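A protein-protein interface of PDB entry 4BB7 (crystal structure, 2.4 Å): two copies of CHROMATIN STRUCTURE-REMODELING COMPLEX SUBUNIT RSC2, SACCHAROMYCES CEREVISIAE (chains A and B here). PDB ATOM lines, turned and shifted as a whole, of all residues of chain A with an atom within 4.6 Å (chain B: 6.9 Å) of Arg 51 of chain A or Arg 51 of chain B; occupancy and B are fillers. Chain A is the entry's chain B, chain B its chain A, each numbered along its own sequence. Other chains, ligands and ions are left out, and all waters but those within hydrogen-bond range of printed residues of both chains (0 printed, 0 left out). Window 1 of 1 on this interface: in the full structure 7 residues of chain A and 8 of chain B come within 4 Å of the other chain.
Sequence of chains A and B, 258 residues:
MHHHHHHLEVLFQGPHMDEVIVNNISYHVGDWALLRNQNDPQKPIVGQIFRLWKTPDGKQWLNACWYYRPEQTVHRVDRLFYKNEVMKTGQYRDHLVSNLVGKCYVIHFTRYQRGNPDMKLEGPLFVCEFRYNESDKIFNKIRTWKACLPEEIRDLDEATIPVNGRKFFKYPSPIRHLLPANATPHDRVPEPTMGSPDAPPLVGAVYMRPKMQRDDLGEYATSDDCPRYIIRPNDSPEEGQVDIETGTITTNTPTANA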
ATOM      1  N   PRO A  15     -21.562 -15.887  25.321  1.00  0.00           N
ATOM      2  CA  PRO A  15     -21.133 -15.647  23.942  1.00  0.00           C
ATOM      3  C   PRO A  15     -21.600 -14.293  23.430  1.00  0.00           C
ATOM      4  O   PRO A  15     -22.173 -14.209  22.342  1.00  0.00           O
ATOM      5  CB  PRO A  15     -21.850 -16.748  23.170  1.00  0.00           C
ATOM      6  CG  PRO A  15     -23.086 -16.986  23.940  1.00  0.00           C
ATOM      7  CD  PRO A  15     -22.693 -16.830  25.384  1.00  0.00           C
ATOM      8  N   VAL A  29     -11.437 -13.971  27.132  1.00  0.00           N
ATOM      9  CA  VAL A  29     -11.508 -15.422  27.160  1.00  0.00           C
ATOM     10  C   VAL A  29     -10.098 -15.966  26.995  1.00  0.00           C
ATOM     11  O   VAL A  29      -9.364 -15.539  26.104  1.00  0.00           O
ATOM     12  CB  VAL A  29     -12.423 -15.967  26.047  1.00  0.00           C
ATOM     13  CG1 VAL A  29     -12.203 -17.463  25.850  1.00  0.00           C
ATOM     14  CG2 VAL A  29     -13.880 -15.674  26.371  1.00  0.00           C
ATOM     15  N   ILE A  49     -10.825 -17.907  32.224  1.00  0.00           N
ATOM     16  CA  ILE A  49     -12.097 -17.531  31.613  1.00  0.00           C
ATOM     17  C   ILE A  49     -12.360 -18.256  30.288  1.00  0.00           C
ATOM     18  O   ILE A  49     -11.550 -18.189  29.360  1.00  0.00           O
ATOM     19  CB  ILE A  49     -12.170 -16.010  31.393  1.00  0.00           C
ATOM     20  CG1 ILE A  49     -11.901 -15.279  32.711  1.00  0.00           C
ATOM     21  CG2 ILE A  49     -13.522 -15.620  30.816  1.00  0.00           C
ATOM     22  CD1 ILE A  49     -11.494 -13.833  32.553  1.00  0.00           C
ATOM     23  N   PHE A  50     -13.499 -18.942  30.206  1.00  0.00           N
ATOM     24  CA  PHE A  50     -13.875 -19.685  29.004  1.00  0.00           C
ATOM     25  C   PHE A  50     -14.985 -19.010  28.201  1.00  0.00           C
ATOM     26  O   PHE A  50     -15.128 -19.262  27.002  1.00  0.00           O
ATOM     27  CB  PHE A  50     -14.303 -21.110  29.362  1.00  0.00           C
ATOM     28  CG  PHE A  50     -13.161 -22.078  29.476  1.00  0.00           C
ATOM     29  CD1 PHE A  50     -12.257 -21.985  30.525  1.00  0.00           C
ATOM     30  CD2 PHE A  50     -13.001 -23.093  28.542  1.00  0.00           C
ATOM     31  CE1 PHE A  50     -11.210 -22.875  30.636  1.00  0.00           C
ATOM     32  CE2 PHE A  50     -11.955 -23.992  28.647  1.00  0.00           C
ATOM     33  CZ  PHE A  50     -11.058 -23.882  29.695  1.00  0.00           C
ATOM     34  N   ARG A  51     -15.773 -18.165  28.862  1.00  0.00           N
ATOM     35  CA  ARG A  51     -16.894 -17.495  28.207  1.00  0.00           C
ATOM     36  C   ARG A  51     -17.305 -16.206  28.907  1.00  0.00           C
ATOM     37  O   ARG A  51     -17.342 -16.140  30.136  1.00  0.00           O
ATOM     38  CB  ARG A  51     -18.103 -18.431  28.117  1.00  0.00           C
ATOM     39  CG  ARG A  51     -18.208 -19.182  26.801  1.00  0.00           C
ATOM     40  CD  ARG A  51     -19.406 -20.116  26.789  1.00  0.00           C
ATOM     41  NE  ARG A  51     -20.586 -19.488  27.369  1.00  0.00           N
ATOM     42  CZ  ARG A  51     -21.191 -19.913  28.473  1.00  0.00           C
ATOM     43  NH1 ARG A  51     -20.735 -20.982  29.110  1.00  0.00           N
ATOM     44  NH2 ARG A  51     -22.258 -19.273  28.934  1.00  0.00           N
ATOM     45  N   LEU A  52     -17.620 -15.188  28.110  1.00  0.00           N
ATOM     46  CA  LEU A  52     -18.167 -13.936  28.622  1.00  0.00           C
ATOM     47  C   LEU A  52     -19.549 -13.692  28.028  1.00  0.00           C
ATOM     48  O   LEU A  52     -19.849 -14.153  26.928  1.00  0.00           O
ATOM     49  CB  LEU A  52     -17.251 -12.762  28.267  1.00  0.00           C
ATOM     50  CG  LEU A  52     -15.808 -12.815  28.777  1.00  0.00           C
ATOM     51  CD1 LEU A  52     -14.979 -11.692  28.167  1.00  0.00           C
ATOM     52  CD2 LEU A  52     -15.770 -12.752  30.295  1.00  0.00           C
ATOM     53  N   TRP A  53     -20.392 -12.968  28.756  1.00  0.00           N
ATOM     54  CA  TRP A  53     -21.686 -12.564  28.219  1.00  0.00           C
ATOM     55  C   TRP A  53     -22.435 -11.600  29.136  1.00  0.00           C
ATOM     56  O   TRP A  53     -22.097 -11.439  30.309  1.00  0.00           O
ATOM     57  CB  TRP A  53     -22.562 -13.781  27.923  1.00  0.00           C
ATOM     58  CG  TRP A  53     -23.107 -14.434  29.148  1.00  0.00           C
ATOM     59  CD1 TRP A  53     -24.343 -14.248  29.695  1.00  0.00           C
ATOM     60  CD2 TRP A  53     -22.434 -15.378  29.989  1.00  0.00           C
ATOM     61  NE1 TRP A  53     -24.483 -15.021  30.820  1.00  0.00           N
ATOM     62  CE2 TRP A  53     -23.324 -15.723  31.025  1.00  0.00           C
ATOM     63  CE3 TRP A  53     -21.165 -15.965  29.965  1.00  0.00           C
ATOM     64  CZ2 TRP A  53     -22.988 -16.632  32.029  1.00  0.00           C
ATOM     65  CZ3 TRP A  53     -20.831 -16.864  30.961  1.00  0.00           C
ATOM     66  CH2 TRP A  53     -21.741 -17.191  31.980  1.00  0.00           C
ATOM     67  N   THR A  55     -26.309 -10.563  30.596  1.00  0.00           N
ATOM     68  CA  THR A  55     -27.649 -11.098  30.810  1.00  0.00           C
ATOM     69  C   THR A  55     -28.695 -10.004  30.615  1.00  0.00           C
ATOM     70  O   THR A  55     -28.357  -8.822  30.597  1.00  0.00           O
ATOM     71  CB  THR A  55     -27.792 -11.729  32.211  1.00  0.00           C
ATOM     72  OG1 THR A  55     -27.343 -10.801  33.202  1.00  0.00           O
ATOM     73  CG2 THR A  55     -26.969 -13.005  32.309  1.00  0.00           C
ATOM     74  N   TRP A  61     -21.342 -11.271  32.814  1.00  0.00           N
ATOM     75  CA  TRP A  61     -21.056 -12.593  33.364  1.00  0.00           C
ATOM     76  C   TRP A  61     -19.900 -13.291  32.663  1.00  0.00           C
ATOM     77  O   TRP A  61     -19.510 -12.920  31.556  1.00  0.00           O
ATOM     78  CB  TRP A  61     -22.295 -13.477  33.273  1.00  0.00           C
ATOM     79  CG  TRP A  61     -23.356 -13.112  34.248  1.00  0.00           C
ATOM     80  CD1 TRP A  61     -24.260 -12.096  34.140  1.00  0.00           C
ATOM     81  CD2 TRP A  61     -23.636 -13.770  35.486  1.00  0.00           C
ATOM     82  NE1 TRP A  61     -25.083 -12.076  35.237  1.00  0.00           N
ATOM     83  CE2 TRP A  61     -24.723 -13.094  36.079  1.00  0.00           C
ATOM     84  CE3 TRP A  61     -23.070 -14.863  36.154  1.00  0.00           C
ATOM     85  CZ2 TRP A  61     -25.256 -13.476  37.307  1.00  0.00           C
ATOM     86  CZ3 TRP A  61     -23.601 -15.241  37.374  1.00  0.00           C
ATOM     87  CH2 TRP A  61     -24.683 -14.549  37.938  1.00  0.00           C
ATOM     88  N   LEU A  62     -19.368 -14.320  33.310  1.00  0.00           N
ATOM     89  CA  LEU A  62     -18.237 -15.060  32.772  1.00  0.00           C
ATOM     90  C   LEU A  62     -18.243 -16.486  33.280  1.00  0.00           C
ATOM     91  O   LEU A  62     -18.856 -16.790  34.302  1.00  0.00           O
ATOM     92  CB  LEU A  62     -16.911 -14.384  33.154  1.00  0.00           C
ATOM     93  CG  LEU A  62     -16.492 -14.421  34.627  1.00  0.00           C
ATOM     94  CD1 LEU A  62     -15.891 -15.769  35.001  1.00  0.00           C
ATOM     95  CD2 LEU A  62     -15.509 -13.305  34.929  1.00  0.00           C
ATOM     96  N   ASN A  63     -17.552 -17.358  32.559  1.00  0.00           N
ATOM     97  CA  ASN A  63     -17.385 -18.734  32.995  1.00  0.00           C
ATOM     98  C   ASN A  63     -15.906 -19.095  33.068  1.00  0.00           C
ATOM     99  O   ASN A  63     -15.176 -18.971  32.088  1.00  0.00           O
ATOM    100  CB  ASN A  63     -18.144 -19.693  32.070  1.00  0.00           C
ATOM    101  CG  ASN A  63     -18.010 -21.146  32.499  1.00  0.00           C
ATOM    102  OD1 ASN A  63     -17.152 -21.874  31.999  1.00  0.00           O
ATOM    103  ND2 ASN A  63     -18.856 -21.570  33.431  1.00  0.00           N
ATOM    104  N   HIS B  16     -22.213 -19.197  21.839  1.00  0.00           N
ATOM    105  CA  HIS B  16     -21.385 -18.832  20.697  1.00  0.00           C
ATOM    106  C   HIS B  16     -21.917 -19.519  19.448  1.00  0.00           C
ATOM    107  O   HIS B  16     -21.295 -19.482  18.389  1.00  0.00           O
ATOM    108  CB  HIS B  16     -19.925 -19.219  20.946  1.00  0.00           C
ATOM    109  N   MET B  17     -23.079 -20.149  19.592  1.00  0.00           N
ATOM    110  CA  MET B  17     -23.741 -20.812  18.479  1.00  0.00           C
ATOM    111  C   MET B  17     -24.697 -19.852  17.783  1.00  0.00           C
ATOM    112  O   MET B  17     -25.138 -18.859  18.366  1.00  0.00           O
ATOM    113  CB  MET B  17     -24.502 -22.047  18.968  1.00  0.00           C
ATOM    114  CG  MET B  17     -23.626 -23.064  19.688  1.00  0.00           C
ATOM    115  SD  MET B  17     -24.507 -24.569  20.156  1.00  0.00           S
ATOM    116  CE  MET B  17     -25.696 -23.933  21.335  1.00  0.00           C
ATOM    117  N   VAL B  29     -32.025 -17.775  18.804  1.00  0.00           N
ATOM    118  CA  VAL B  29     -32.322 -16.830  19.872  1.00  0.00           C
ATOM    119  C   VAL B  29     -33.561 -16.017  19.507  1.00  0.00           C
ATOM    120  O   VAL B  29     -33.710 -15.575  18.370  1.00  0.00           O
ATOM    121  CB  VAL B  29     -31.136 -15.880  20.144  1.00  0.00           C
ATOM    122  CG1 VAL B  29     -31.478 -14.904  21.259  1.00  0.00           C
ATOM    123  CG2 VAL B  29     -29.895 -16.680  20.497  1.00  0.00           C
ATOM    124  N   GLY B  30     -34.448 -15.832  20.475  1.00  0.00           N
ATOM    125  CA  GLY B  30     -35.666 -15.080  20.253  1.00  0.00           C
ATOM    126  C   GLY B  30     -36.811 -15.997  19.879  1.00  0.00           C
ATOM    127  O   GLY B  30     -37.948 -15.552  19.711  1.00  0.00           O
ATOM    128  N   GLN B  48     -38.701 -18.995  25.863  1.00  0.00           N
ATOM    129  CA  GLN B  48     -38.110 -18.319  24.714  1.00  0.00           C
ATOM    130  C   GLN B  48     -36.588 -18.341  24.825  1.00  0.00           C
ATOM    131  O   GLN B  48     -36.036 -18.033  25.880  1.00  0.00           O
ATOM    132  CB  GLN B  48     -38.609 -16.877  24.611  1.00  0.00           C
ATOM    133  CG  GLN B  48     -38.018 -16.112  23.432  1.00  0.00           C
ATOM    134  CD  GLN B  48     -38.581 -14.711  23.289  1.00  0.00           C
ATOM    135  OE1 GLN B  48     -38.988 -14.087  24.267  1.00  0.00           O
ATOM    136  NE2 GLN B  48     -38.606 -14.212  22.061  1.00  0.00           N
ATOM    137  N   ILE B  49     -35.914 -18.703  23.739  1.00  0.00           N
ATOM    138  CA  ILE B  49     -34.458 -18.811  23.746  1.00  0.00           C
ATOM    139  C   ILE B  49     -33.736 -17.457  23.781  1.00  0.00           C
ATOM    140  O   ILE B  49     -33.815 -16.674  22.837  1.00  0.00           O
ATOM    141  CB  ILE B  49     -33.961 -19.621  22.543  1.00  0.00           C
ATOM    142  CG1 ILE B  49     -34.595 -21.014  22.560  1.00  0.00           C
ATOM    143  CG2 ILE B  49     -32.444 -19.716  22.558  1.00  0.00           C
ATOM    144  CD1 ILE B  49     -34.396 -21.798  21.282  1.00  0.00           C
ATOM    145  N   PHE B  50     -33.026 -17.194  24.872  1.00  0.00           N
ATOM    146  CA  PHE B  50     -32.280 -15.944  25.012  1.00  0.00           C
ATOM    147  C   PHE B  50     -30.825 -16.056  24.557  1.00  0.00           C
ATOM    148  O   PHE B  50     -30.231 -15.066  24.130  1.00  0.00           O
ATOM    149  CB  PHE B  50     -32.335 -15.435  26.453  1.00  0.00           C
ATOM    150  CG  PHE B  50     -33.509 -14.548  26.741  1.00  0.00           C
ATOM    151  CD1 PHE B  50     -34.800 -15.062  26.760  1.00  0.00           C
ATOM    152  CD2 PHE B  50     -33.324 -13.199  27.008  1.00  0.00           C
ATOM    153  CE1 PHE B  50     -35.885 -14.241  27.031  1.00  0.00           C
ATOM    154  CE2 PHE B  50     -34.402 -12.376  27.279  1.00  0.00           C
ATOM    155  CZ  PHE B  50     -35.685 -12.898  27.290  1.00  0.00           C
ATOM    156  N   ARG B  51     -30.244 -17.248  24.665  1.00  0.00           N
ATOM    157  CA  ARG B  51     -28.881 -17.455  24.185  1.00  0.00           C
ATOM    158  C   ARG B  51     -28.515 -18.934  24.073  1.00  0.00           C
ATOM    159  O   ARG B  51     -29.119 -19.785  24.723  1.00  0.00           O
ATOM    160  CB  ARG B  51     -27.865 -16.711  25.064  1.00  0.00           C
ATOM    161  CG  ARG B  51     -27.444 -17.464  26.307  1.00  0.00           C
ATOM    162  CD  ARG B  51     -26.391 -16.697  27.093  1.00  0.00           C
ATOM    163  NE  ARG B  51     -25.857 -17.489  28.199  1.00  0.00           N
ATOM    164  CZ  ARG B  51     -26.364 -17.497  29.428  1.00  0.00           C
ATOM    165  NH1 ARG B  51     -27.425 -16.748  29.713  1.00  0.00           N
ATOM    166  NH2 ARG B  51     -25.813 -18.255  30.372  1.00  0.00           N
ATOM    167  N   LEU B  52     -27.524 -19.220  23.234  1.00  0.00           N
ATOM    168  CA  LEU B  52     -27.063 -20.581  22.993  1.00  0.00           C
ATOM    169  C   LEU B  52     -25.540 -20.615  23.033  1.00  0.00           C
ATOM    170  O   LEU B  52     -24.885 -19.628  22.699  1.00  0.00           O
ATOM    171  CB  LEU B  52     -27.538 -21.066  21.621  1.00  0.00           C
ATOM    172  CG  LEU B  52     -29.032 -21.040  21.297  1.00  0.00           C
ATOM    173  CD1 LEU B  52     -29.248 -20.871  19.796  1.00  0.00           C
ATOM    174  CD2 LEU B  52     -29.733 -22.291  21.810  1.00  0.00           C
ATOM    175  N   TRP B  53     -24.975 -21.751  23.430  1.00  0.00           N
ATOM    176  CA  TRP B  53     -23.527 -21.892  23.484  1.00  0.00           C
ATOM    177  C   TRP B  53     -23.106 -23.342  23.673  1.00  0.00           C
ATOM    178  O   TRP B  53     -23.913 -24.191  24.043  1.00  0.00           O
ATOM    179  CB  TRP B  53     -22.950 -21.043  24.615  1.00  0.00           C
ATOM    180  CG  TRP B  53     -23.225 -21.599  25.975  1.00  0.00           C
ATOM    181  CD1 TRP B  53     -22.418 -22.428  26.702  1.00  0.00           C
ATOM    182  CD2 TRP B  53     -24.390 -21.371  26.778  1.00  0.00           C
ATOM    183  NE1 TRP B  53     -23.007 -22.727  27.907  1.00  0.00           N
ATOM    184  CE2 TRP B  53     -24.218 -22.091  27.979  1.00  0.00           C
ATOM    185  CE3 TRP B  53     -25.559 -20.627  26.599  1.00  0.00           C
ATOM    186  CZ2 TRP B  53     -25.172 -22.088  28.995  1.00  0.00           C
ATOM    187  CZ3 TRP B  53     -26.504 -20.626  27.608  1.00  0.00           C
ATOM    188  CH2 TRP B  53     -26.306 -21.352  28.791  1.00  0.00           C
ATOM    189  N   LYS B  54     -21.832 -23.614  23.419  1.00  0.00           N
ATOM    190  CA  LYS B  54     -21.283 -24.955  23.573  1.00  0.00           C
ATOM    191  C   LYS B  54     -20.264 -24.984  24.706  1.00  0.00           C
ATOM    192  O   LYS B  54     -19.430 -24.087  24.830  1.00  0.00           O
ATOM    193  CB  LYS B  54     -20.632 -25.416  22.268  1.00  0.00           C
ATOM    194  CG  LYS B  54     -20.006 -26.797  22.338  1.00  0.00           C
ATOM    195  CD  LYS B  54     -19.308 -27.148  21.033  1.00  0.00           C
ATOM    196  CE  LYS B  54     -18.199 -26.156  20.715  1.00  0.00           C
ATOM    197  NZ  LYS B  54     -17.512 -26.471  19.430  1.00  0.00           N
ATOM    198  N   THR B  55     -20.339 -26.016  25.539  1.00  0.00           N
ATOM    199  CA  THR B  55     -19.412 -26.163  26.654  1.00  0.00           C
ATOM    200  C   THR B  55     -18.204 -27.002  26.234  1.00  0.00           C
ATOM    201  O   THR B  55     -18.276 -27.742  25.252  1.00  0.00           O
ATOM    202  CB  THR B  55     -20.108 -26.771  27.890  1.00  0.00           C
ATOM    203  OG1 THR B  55     -20.875 -27.916  27.497  1.00  0.00           O
ATOM    204  CG2 THR B  55     -21.037 -25.751  28.522  1.00  0.00           C
ATOM    205  N   PRO B  56     -17.085 -26.876  26.969  1.00  0.00           N
ATOM    206  CA  PRO B  56     -15.826 -27.541  26.613  1.00  0.00           C
ATOM    207  C   PRO B  56     -15.999 -29.005  26.216  1.00  0.00           C
ATOM    208  O   PRO B  56     -15.246 -29.496  25.379  1.00  0.00           O
ATOM    209  CB  PRO B  56     -15.003 -27.429  27.898  1.00  0.00           C
ATOM    210  CG  PRO B  56     -15.465 -26.153  28.503  1.00  0.00           C
ATOM    211  CD  PRO B  56     -16.942 -26.062  28.190  1.00  0.00           C
ATOM    212  N   TRP B  61     -25.884 -25.906  24.882  1.00  0.00           N
ATOM    213  CA  TRP B  61     -26.786 -25.383  25.897  1.00  0.00           C
ATOM    214  C   TRP B  61     -27.579 -24.175  25.403  1.00  0.00           C
ATOM    215  O   TRP B  61     -27.275 -23.590  24.363  1.00  0.00           O
ATOM    216  CB  TRP B  61     -25.993 -24.977  27.139  1.00  0.00           C
ATOM    217  CG  TRP B  61     -25.530 -26.117  27.985  1.00  0.00           C
ATOM    218  CD1 TRP B  61     -24.487 -26.960  27.728  1.00  0.00           C
ATOM    219  CD2 TRP B  61     -26.077 -26.526  29.245  1.00  0.00           C
ATOM    220  NE1 TRP B  61     -24.356 -27.875  28.746  1.00  0.00           N
ATOM    221  CE2 TRP B  61     -25.318 -27.629  29.691  1.00  0.00           C
ATOM    222  CE3 TRP B  61     -27.133 -26.067  30.038  1.00  0.00           C
ATOM    223  CZ2 TRP B  61     -25.586 -28.283  30.893  1.00  0.00           C
ATOM    224  CZ3 TRP B  61     -27.400 -26.718  31.228  1.00  0.00           C
ATOM    225  CH2 TRP B  61     -26.629 -27.816  31.645  1.00  0.00           C
ATOM    226  N   LEU B  62     -28.592 -23.804  26.175  1.00  0.00           N
ATOM    227  CA  LEU B  62     -29.396 -22.630  25.879  1.00  0.00           C
ATOM    228  C   LEU B  62     -29.903 -22.004  27.170  1.00  0.00           C
ATOM    229  O   LEU B  62     -29.975 -22.661  28.210  1.00  0.00           O
ATOM    230  CB  LEU B  62     -30.569 -23.000  24.967  1.00  0.00           C
ATOM    231  CG  LEU B  62     -31.560 -24.058  25.459  1.00  0.00           C
ATOM    232  CD1 LEU B  62     -32.553 -23.453  26.447  1.00  0.00           C
ATOM    233  CD2 LEU B  62     -32.297 -24.679  24.281  1.00  0.00           C
ATOM    234  N   ASN B  63     -30.247 -20.725  27.100  1.00  0.00           N
ATOM    235  CA  ASN B  63     -30.868 -20.052  28.225  1.00  0.00           C
ATOM    236  C   ASN B  63     -32.255 -19.539  27.855  1.00  0.00           C
ATOM    237  O   ASN B  63     -32.401 -18.642  27.019  1.00  0.00           O
ATOM    238  CB  ASN B  63     -29.985 -18.910  28.724  1.00  0.00           C
ATOM    239  CG  ASN B  63     -30.581 -18.201  29.919  1.00  0.00           C
ATOM    240  OD1 ASN B  63     -31.419 -17.314  29.770  1.00  0.00           O
ATOM    241  ND2 ASN B  63     -30.155 -18.593  31.116  1.00  0.00           N
ATOM    242  N   ALA B  64     -33.276 -20.119  28.476  1.00  0.00           N
ATOM    243  CA  ALA B  64     -34.655 -19.749  28.178  1.00  0.00           C
ATOM    244  C   ALA B  64     -35.339 -19.045  29.350  1.00  0.00           C
ATOM    245  O   ALA B  64     -35.084 -19.361  30.513  1.00  0.00           O
ATOM    246  CB  ALA B  64     -35.448 -20.978  27.759  1.00  0.00           C
ATOM    247  N   TYR B  92     -34.770 -17.380  34.333  1.00  0.00           N
ATOM    248  CA  TYR B  92     -33.920 -17.578  33.162  1.00  0.00           C
ATOM    249  C   TYR B  92     -33.015 -18.777  33.411  1.00  0.00           C
ATOM    250  O   TYR B  92     -31.985 -18.664  34.073  1.00  0.00           O
ATOM    251  CB  TYR B  92     -33.107 -16.316  32.854  1.00  0.00           C
ATOM    252  CG  TYR B  92     -33.972 -15.103  32.577  1.00  0.00           C
ATOM    253  CD1 TYR B  92     -34.564 -14.398  33.618  1.00  0.00           C
ATOM    254  CD2 TYR B  92     -34.202 -14.667  31.280  1.00  0.00           C
ATOM    255  CE1 TYR B  92     -35.359 -13.290  33.377  1.00  0.00           C
ATOM    256  CE2 TYR B  92     -34.998 -13.559  31.026  1.00  0.00           C
ATOM    257  CZ  TYR B  92     -35.576 -12.874  32.080  1.00  0.00           C
ATOM    258  OH  TYR B  92     -36.369 -11.769  31.842  1.00  0.00           O
ATOM    259  N   ARG B  93     -33.417 -19.929  32.887  1.00  0.00           N
ATOM    260  CA  ARG B  93     -32.748 -21.188  33.197  1.00  0.00           C
ATOM    261  C   ARG B  93     -31.933 -21.721  32.027  1.00  0.00           C
ATOM    262  O   ARG B  93     -32.235 -21.443  30.868  1.00  0.00           O
ATOM    263  CB  ARG B  93     -33.775 -22.239  33.625  1.00  0.00           C
ATOM    264  CG  ARG B  93     -34.425 -21.985  34.978  1.00  0.00           C
ATOM    265  CD  ARG B  93     -33.394 -22.027  36.095  1.00  0.00           C
ATOM    266  NE  ARG B  93     -34.015 -22.053  37.415  1.00  0.00           N
ATOM    267  CZ  ARG B  93     -34.179 -23.153  38.142  1.00  0.00           C
ATOM    268  NH1 ARG B  93     -33.763 -24.324  37.684  1.00  0.00           N
ATOM    269  NH2 ARG B  93     -34.754 -23.080  39.333  1.00  0.00           N
ATOM    270  N   ASP B  94     -30.900 -22.493  32.344  1.00  0.00           N
ATOM    271  CA  ASP B  94     -30.076 -23.142  31.332  1.00  0.00           C
ATOM    272  C   ASP B  94     -30.556 -24.569  31.085  1.00  0.00           C
ATOM    273  O   ASP B  94     -30.825 -25.311  32.031  1.00  0.00           O
ATOM    274  CB  ASP B  94     -28.608 -23.166  31.766  1.00  0.00           C
ATOM    275  CG  ASP B  94     -28.002 -21.777  31.859  1.00  0.00           C
ATOM    276  OD1 ASP B  94     -28.586 -20.831  31.291  1.00  0.00           O
ATOM    277  OD2 ASP B  94     -26.934 -21.635  32.491  1.00  0.00           O
ATOM    278  N   PRO B 150     -35.518 -10.926  24.138  1.00  0.00           N
ATOM    279  CA  PRO B 150     -34.057 -10.835  24.060  1.00  0.00           C
ATOM    280  C   PRO B 150     -33.659  -9.556  23.331  1.00  0.00           C
ATOM    281  O   PRO B 150     -34.341  -9.138  22.393  1.00  0.00           O
ATOM    282  CB  PRO B 150     -33.668 -12.064  23.230  1.00  0.00           C
ATOM    283  CG  PRO B 150     -34.821 -12.997  23.364  1.00  0.00           C
ATOM    284  CD  PRO B 150     -36.033 -12.123  23.454  1.00  0.00           C
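NE1 of Trp 53 of chain B lies close to NH1 of Arg 51 of chain A (3.1 Å).
N of His 16 of chain B is in hydrogen-bond range of O of Leu 52 of chain B, 2.8 Å away. The backbone carbonyl oxygen of Arg 51 of chain B is in hydrogen-bond range of the backbone NH of Asn 63 of chain B (2.8 Å). NH2 of Arg 51 of chain B is in salt-bridge range of OD1 of Asp 94 of chain B, 3.9 Å away. The backbone NH of Trp 61 of chain B sits at hydrogen-bond distance from the backbone carbonyl oxygen of Trp 53 of chain B (2.7 Å). N of Phe 50 of chain A sits at hydrogen-bond distance from O of Asn 63 of chain A (2.5 Å). The backbone NH of Asn 63 of chain A sits at hydrogen-bond distance from the backbone carbonyl oxygen of Arg 51 of chain A.
Among the printed residues, pairs that only touch across the chains: Pro 15 of chain A with His 16 of chain B (2.8 Å), Pro 15 of chain A with Leu 52 of chain B (3.4 Å), Phe 50 of chain A with Pro 56 of chain B (3.9 Å), Arg 51 of chain A with Arg 51 of chain B (3.97 Å) and Trp 53 of chain A with Arg 51 of chain B (3.4 Å).
Of chain B, only Arg 51 (3.97 Å) and Trp 53 (3.1 Å) come within 4 Å of Arg 51 of chain A. Arg 51 of chain B touches just these residues of chain A: Arg 51 (3.97 Å) and Trp 53 (3.4 Å). Of the printed residues of chain A, Leu 52 of chain B touches Pro 15. Printed residues of chain A within 4 Å of Trp 53 of chain B: Arg 51 (3.1 Å). Of the printed residues of chain A, Pro 56 of chain B touches Phe 50 (3.9 Å). The nearest residue of chain A that does not touch Arg 51 of chain B is Pro 15 of chain A (4.1 Å). The nearest printed residue of chain A that does not touch His 16 of chain B is Arg 51 of chain A (5.8 Å).
Of the 11 printed residues of chain A, 4 touch a printed residue of chain B. Hydrophobic or aromatic side chains of chain B within 4 Å of the printed part of chain A: His 16, Trp 53 and Pro 56. Along chain B the printed residues that touch a printed residue of chain A span positions 16 to 56. Among the printed residues, no Asp or Glu carboxylate lies within 4 Å of a Lys or Arg side-chain nitrogen of the other chain.
Arg 51 of chain B touches its own counterpart, Arg 51 of chain A. Arg 51 of chain A touches Trp 53 of chain B, and with the chains exchanged Trp 53 of chain A touches Arg 51 of chain B. Of the 6 pairs that touch across the chains among the printed residues, 3 have their exchanged pair printed and touching as well.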
